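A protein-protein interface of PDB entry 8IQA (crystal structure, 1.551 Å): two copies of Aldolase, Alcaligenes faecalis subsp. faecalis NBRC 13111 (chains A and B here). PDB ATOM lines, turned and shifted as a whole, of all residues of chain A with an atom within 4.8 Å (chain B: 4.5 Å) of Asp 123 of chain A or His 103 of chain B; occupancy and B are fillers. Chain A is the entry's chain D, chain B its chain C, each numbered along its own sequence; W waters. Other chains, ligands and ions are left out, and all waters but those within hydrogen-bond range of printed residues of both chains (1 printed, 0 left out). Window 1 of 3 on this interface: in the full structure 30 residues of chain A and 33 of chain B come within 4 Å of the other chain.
ND1 of His 103 of chain B lies within hydrogen-bond range of OD2 of Asp 123 of chain A, 2.6 Å away.
O of His 165 of chain B lies within hydrogen-bond range of NE2 of Gln 121 of chain A (2.9 Å).
SD of Met 124 of chain A sits at hydrogen-bond distance from N of Gln 121 of chain A (3.7 Å).
OE1 of Gln 121 of chain A sits at hydrogen-bond distance from N of Asp 123 of chain A (2.9 Å).
The backbone carbonyl oxygen (O) of Ser 104 of chain B is in hydrogen-bond range of the side-chain hydroxyl (OG1) of Thr 108 of chain B, at 2.7 Å.
Among the printed residues, merely in contact across the chains: Gln 121 of chain A with His 103 of chain B (3.8 Å), Gln 121 of chain A with Thr 108 of chain B (3.5 Å) and Tyr 183 of chain A with Ala 30 of chain B (3.97 Å).
Of chain B, only His 103 (2.6 Å) comes within 4 Å of Asp 123 of chain A.
His 103 of chain B touches just these residues of chain A: Gln 121 and Asp 123.
Of the printed residues of chain B, Tyr 183 of chain A touches Ala 30 (3.97 Å).
Printed residues of chain B within 4 Å of Gln 121 of chain A: His 103 (3.8 Å), Thr 108 (3.5 Å) and His 165 (2.9 Å).
Of the printed residues of chain A, Ala 30 of chain B touches Tyr 183 (3.97 Å).
Of the printed residues of chain A, Thr 108 of chain B touches Gln 121 (3.5 Å).
Of the printed residues of chain A, His 165 of chain B touches Gln 121.
Thr 102 of chain B touches none of the printed residues of chain A.
Leu 216 of chain A touches none of the printed residues of chain B.
The nearest residue of chain A that does not touch His 103 of chain B is Met 122 of chain A (4.1 Å).
The nearest printed residue of chain B that does not touch Tyr 183 of chain A is Ala 33 of chain B (5.7 Å).
Of the 8 printed residues of chain A, 3 touch a printed residue of chain B.
Hydrophobic or aromatic side chains of chain A that line the printed part of chain B: Tyr 183.
No position is printed for both chains.
Of the 5 pairs that touch across the chains among the printed residues, none has its exchanged pair printed and touching as well.
Water W1 lies within hydrogen-bond range of the side-chain hydroxyl (OH) of Tyr 183 of chain A (2.7 Å), the side-chain carboxylate (OD1) of Asp 123 of chain A (2.8 Å) and the backbone carbonyl oxygen (O) of Ala 30 of chain B (2.9 Å).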
ATOM      1  N   GLN A 121     -16.640 -23.513 -23.879  1.00  0.00           N
ATOM      2  CA  GLN A 121     -16.190 -22.722 -25.026  1.00  0.00           C
ATOM      3  C   GLN A 121     -14.929 -21.954 -24.644  1.00  0.00           C
ATOM      4  O   GLN A 121     -14.729 -21.610 -23.481  1.00  0.00           O
ATOM      5  CB  GLN A 121     -17.307 -21.753 -25.478  1.00  0.00           C
ATOM      6  CG  GLN A 121     -17.008 -20.973 -26.750  1.00  0.00           C
ATOM      7  CD  GLN A 121     -16.503 -19.560 -26.505  1.00  0.00           C
ATOM      8  OE1 GLN A 121     -16.551 -19.042 -25.372  1.00  0.00           O
ATOM      9  NE2 GLN A 121     -15.935 -18.919 -27.538  1.00  0.00           N
ATOM     10  N   MET A 122     -14.063 -21.713 -25.623  1.00  0.00           N
ATOM     11  CA  MET A 122     -12.774 -21.033 -25.479  1.00  0.00           C
ATOM     12  C   MET A 122     -12.796 -19.812 -24.517  1.00  0.00           C
ATOM     13  O   MET A 122     -11.962 -19.736 -23.618  1.00  0.00           O
ATOM     14  CB  MET A 122     -12.283 -20.619 -26.892  1.00  0.00           C
ATOM     15  CG  MET A 122     -11.113 -19.696 -26.881  1.00  0.00           C
ATOM     16  SD  MET A 122      -9.673 -20.594 -26.247  1.00  0.00           S
ATOM     17  CE  MET A 122      -8.371 -19.424 -26.736  1.00  0.00           C
ATOM     18  N   ASP A 123     -13.697 -18.841 -24.735  1.00  0.00           N
ATOM     19  CA  ASP A 123     -13.739 -17.639 -23.927  1.00  0.00           C
ATOM     20  C   ASP A 123     -14.265 -17.856 -22.508  1.00  0.00           C
ATOM     21  O   ASP A 123     -14.221 -16.920 -21.712  1.00  0.00           O
ATOM     22  CB  ASP A 123     -14.532 -16.535 -24.649  1.00  0.00           C
ATOM     23  CG  ASP A 123     -13.938 -16.257 -26.019  1.00  0.00           C
ATOM     24  OD1 ASP A 123     -12.693 -16.143 -26.113  1.00  0.00           O
ATOM     25  OD2 ASP A 123     -14.704 -16.170 -26.979  1.00  0.00           O
ATOM     26  N   MET A 124     -14.829 -19.030 -22.204  1.00  0.00           N
ATOM     27  CA  MET A 124     -15.282 -19.326 -20.840  1.00  0.00           C
ATOM     28  C   MET A 124     -14.088 -19.815 -19.967  1.00  0.00           C
ATOM     29  O   MET A 124     -14.183 -19.824 -18.730  1.00  0.00           O
ATOM     30  CB  MET A 124     -16.352 -20.435 -20.844  1.00  0.00           C
ATOM     31  CG  MET A 124     -17.577 -20.104 -21.731  1.00  0.00           C
ATOM     32  SD  MET A 124     -18.810 -21.438 -21.708  1.00  0.00           S
ATOM     33  CE  MET A 124     -19.723 -20.971 -20.213  1.00  0.00           C
ATOM     34  N   THR A 125     -12.987 -20.273 -20.613  1.00  0.00           N
ATOM     35  CA  THR A 125     -11.845 -20.876 -19.944  1.00  0.00           C
ATOM     36  C   THR A 125     -11.119 -19.967 -18.947  1.00  0.00           C
ATOM     37  O   THR A 125     -10.582 -20.551 -17.996  1.00  0.00           O
ATOM     38  CB  THR A 125     -10.872 -21.513 -20.927  1.00  0.00           C
ATOM     39  OG1 THR A 125     -10.243 -20.504 -21.716  1.00  0.00           O
ATOM     40  CG2 THR A 125     -11.564 -22.574 -21.784  1.00  0.00           C
ATOM     41  N   PRO A 126     -11.090 -18.610 -19.025  1.00  0.00           N
ATOM     42  CA  PRO A 126     -10.481 -17.847 -17.909  1.00  0.00           C
ATOM     43  C   PRO A 126     -11.171 -18.121 -16.567  1.00  0.00           C
ATOM     44  O   PRO A 126     -10.569 -17.844 -15.530  1.00  0.00           O
ATOM     45  CB  PRO A 126     -10.679 -16.378 -18.340  1.00  0.00           C
ATOM     46  CG  PRO A 126     -10.696 -16.454 -19.862  1.00  0.00           C
ATOM     47  CD  PRO A 126     -11.546 -17.694 -20.088  1.00  0.00           C
ATOM     48  N   TYR A 183     -15.559 -11.205 -19.347  1.00  0.00           N
ATOM     49  CA  TYR A 183     -15.573 -12.596 -19.803  1.00  0.00           C
ATOM     50  C   TYR A 183     -16.603 -13.422 -19.042  1.00  0.00           C
ATOM     51  O   TYR A 183     -17.276 -14.246 -19.653  1.00  0.00           O
ATOM     52  CB  TYR A 183     -14.153 -13.229 -19.727  1.00  0.00           C
ATOM     53  CG  TYR A 183     -13.340 -12.912 -20.963  1.00  0.00           C
ATOM     54  CD1 TYR A 183     -12.938 -11.611 -21.245  1.00  0.00           C
ATOM     55  CD2 TYR A 183     -13.046 -13.897 -21.894  1.00  0.00           C
ATOM     56  CE1 TYR A 183     -12.194 -11.311 -22.392  1.00  0.00           C
ATOM     57  CE2 TYR A 183     -12.295 -13.618 -23.034  1.00  0.00           C
ATOM     58  CZ  TYR A 183     -11.907 -12.311 -23.304  1.00  0.00           C
ATOM     59  OH  TYR A 183     -11.225 -12.017 -24.483  1.00  0.00           O
ATOM     60  N   LEU A 216      -5.371 -17.261 -22.179  1.00  0.00           N
ATOM     61  CA  LEU A 216      -6.210 -16.053 -22.174  1.00  0.00           C
ATOM     62  C   LEU A 216      -5.926 -15.111 -21.008  1.00  0.00           C
ATOM     63  O   LEU A 216      -6.350 -13.948 -21.040  1.00  0.00           O
ATOM     64  CB  LEU A 216      -7.678 -16.437 -22.187  1.00  0.00           C
ATOM     65  CG  LEU A 216      -8.172 -16.963 -23.553  1.00  0.00           C
ATOM     66  CD1 LEU A 216      -9.594 -17.400 -23.412  1.00  0.00           C
ATOM     67  CD2 LEU A 216      -8.080 -15.881 -24.630  1.00  0.00           C
ATOM     68  N   ALA B  30     -15.708 -10.248 -29.359  1.00  0.00           N
ATOM     69  CA  ALA B  30     -15.405 -11.093 -28.194  1.00  0.00           C
ATOM     70  C   ALA B  30     -13.952 -10.779 -27.784  1.00  0.00           C
ATOM     71  O   ALA B  30     -13.050 -11.606 -27.981  1.00  0.00           O
ATOM     72  CB  ALA B  30     -15.545 -12.565 -28.577  1.00  0.00           C
ATOM     73  N   ALA B  33     -10.572 -11.502 -30.134  1.00  0.00           N
ATOM     74  CA  ALA B  33     -10.627 -12.803 -30.806  1.00  0.00           C
ATOM     75  C   ALA B  33     -10.779 -12.664 -32.330  1.00  0.00           C
ATOM     76  O   ALA B  33     -10.475 -13.621 -33.028  1.00  0.00           O
ATOM     77  CB  ALA B  33     -11.814 -13.619 -30.292  1.00  0.00           C
ATOM     78  N   HIS B 101     -12.391 -14.974 -38.974  1.00  0.00           N
ATOM     79  CA  HIS B 101     -12.636 -15.862 -37.869  1.00  0.00           C
ATOM     80  C   HIS B 101     -13.052 -14.972 -36.691  1.00  0.00           C
ATOM     81  O   HIS B 101     -12.360 -13.993 -36.374  1.00  0.00           O
ATOM     82  CB  HIS B 101     -11.382 -16.680 -37.465  1.00  0.00           C
ATOM     83  CG  HIS B 101     -11.502 -17.309 -36.095  1.00  0.00           C
ATOM     84  ND1 HIS B 101     -12.430 -18.309 -35.828  1.00  0.00           N
ATOM     85  CD2 HIS B 101     -10.801 -17.059 -34.963  1.00  0.00           C
ATOM     86  CE1 HIS B 101     -12.270 -18.632 -34.548  1.00  0.00           C
ATOM     87  NE2 HIS B 101     -11.308 -17.896 -33.985  1.00  0.00           N
ATOM     88  N   THR B 102     -14.169 -15.305 -36.059  1.00  0.00           N
ATOM     89  CA  THR B 102     -14.604 -14.576 -34.877  1.00  0.00           C
ATOM     90  C   THR B 102     -15.386 -15.570 -33.951  1.00  0.00           C
ATOM     91  O   THR B 102     -15.675 -16.704 -34.338  1.00  0.00           O
ATOM     92  CB  THR B 102     -15.511 -13.308 -35.198  1.00  0.00           C
ATOM     93  OG1 THR B 102     -16.841 -13.757 -35.402  1.00  0.00           O
ATOM     94  CG2 THR B 102     -15.127 -12.551 -36.423  1.00  0.00           C
ATOM     95  N   HIS B 103     -15.670 -15.126 -32.705  1.00  0.00           N
ATOM     96  CA  HIS B 103     -16.468 -15.857 -31.751  1.00  0.00           C
ATOM     97  C   HIS B 103     -17.738 -14.984 -31.567  1.00  0.00           C
ATOM     98  O   HIS B 103     -17.997 -14.439 -30.492  1.00  0.00           O
ATOM     99  CB  HIS B 103     -15.723 -15.967 -30.416  1.00  0.00           C
ATOM    100  CG  HIS B 103     -14.324 -16.502 -30.478  1.00  0.00           C
ATOM    101  ND1 HIS B 103     -13.543 -16.528 -29.332  1.00  0.00           N
ATOM    102  CD2 HIS B 103     -13.600 -16.990 -31.514  1.00  0.00           C
ATOM    103  CE1 HIS B 103     -12.381 -17.059 -29.696  1.00  0.00           C
ATOM    104  NE2 HIS B 103     -12.368 -17.361 -31.000  1.00  0.00           N
ATOM    105  N   SER B 104     -18.499 -14.814 -32.656  1.00  0.00           N
ATOM    106  CA  SER B 104     -19.684 -13.952 -32.628  1.00  0.00           C
ATOM    107  C   SER B 104     -20.762 -14.542 -31.718  1.00  0.00           C
ATOM    108  O   SER B 104     -20.798 -15.746 -31.506  1.00  0.00           O
ATOM    109  CB  SER B 104     -20.189 -13.730 -34.052  1.00  0.00           C
ATOM    110  OG  SER B 104     -20.423 -14.994 -34.644  1.00  0.00           O
ATOM    111  N   PRO B 105     -21.646 -13.708 -31.161  1.00  0.00           N
ATOM    112  CA  PRO B 105     -22.539 -14.207 -30.099  1.00  0.00           C
ATOM    113  C   PRO B 105     -23.401 -15.409 -30.438  1.00  0.00           C
ATOM    114  O   PRO B 105     -23.443 -16.363 -29.665  1.00  0.00           O
ATOM    115  CB  PRO B 105     -23.399 -12.974 -29.731  1.00  0.00           C
ATOM    116  CG  PRO B 105     -22.498 -11.791 -30.056  1.00  0.00           C
ATOM    117  CD  PRO B 105     -21.686 -12.234 -31.268  1.00  0.00           C
ATOM    118  N   THR B 108     -21.513 -18.658 -31.953  1.00  0.00           N
ATOM    119  CA  THR B 108     -20.807 -19.325 -30.874  1.00  0.00           C
ATOM    120  C   THR B 108     -21.750 -20.144 -29.986  1.00  0.00           C
ATOM    121  O   THR B 108     -21.317 -21.169 -29.443  1.00  0.00           O
ATOM    122  CB  THR B 108     -19.943 -18.348 -30.102  1.00  0.00           C
ATOM    123  OG1 THR B 108     -19.067 -17.741 -31.062  1.00  0.00           O
ATOM    124  CG2 THR B 108     -19.113 -19.033 -29.015  1.00  0.00           C
ATOM    125  N   HIS B 165     -15.817 -23.121 -29.775  1.00  0.00           N
ATOM    126  CA  HIS B 165     -14.906 -22.045 -30.137  1.00  0.00           C
ATOM    127  C   HIS B 165     -15.577 -20.879 -30.862  1.00  0.00           C
ATOM    128  O   HIS B 165     -15.671 -19.806 -30.280  1.00  0.00           O
ATOM    129  CB  HIS B 165     -13.748 -22.665 -30.974  1.00  0.00           C
ATOM    130  CG  HIS B 165     -12.665 -21.727 -31.415  1.00  0.00           C
ATOM    131  ND1 HIS B 165     -11.616 -22.184 -32.189  1.00  0.00           N
ATOM    132  CD2 HIS B 165     -12.497 -20.396 -31.188  1.00  0.00           C
ATOM    133  CE1 HIS B 165     -10.838 -21.130 -32.407  1.00  0.00           C
ATOM    134  NE2 HIS B 165     -11.328 -20.028 -31.834  1.00  0.00           N
ATOM    135  N   GLY B 166     -16.009 -21.049 -32.116  1.00  0.00           N
ATOM    136  CA  GLY B 166     -16.552 -19.945 -32.896  1.00  0.00           C
ATOM    137  C   GLY B 166     -16.733 -20.425 -34.323  1.00  0.00           C
ATOM    138  O   GLY B 166     -17.196 -21.555 -34.537  1.00  0.00           O
HETATM  139  O   HOH W   1     -11.643 -13.641 -26.564  1.00  0.00           O
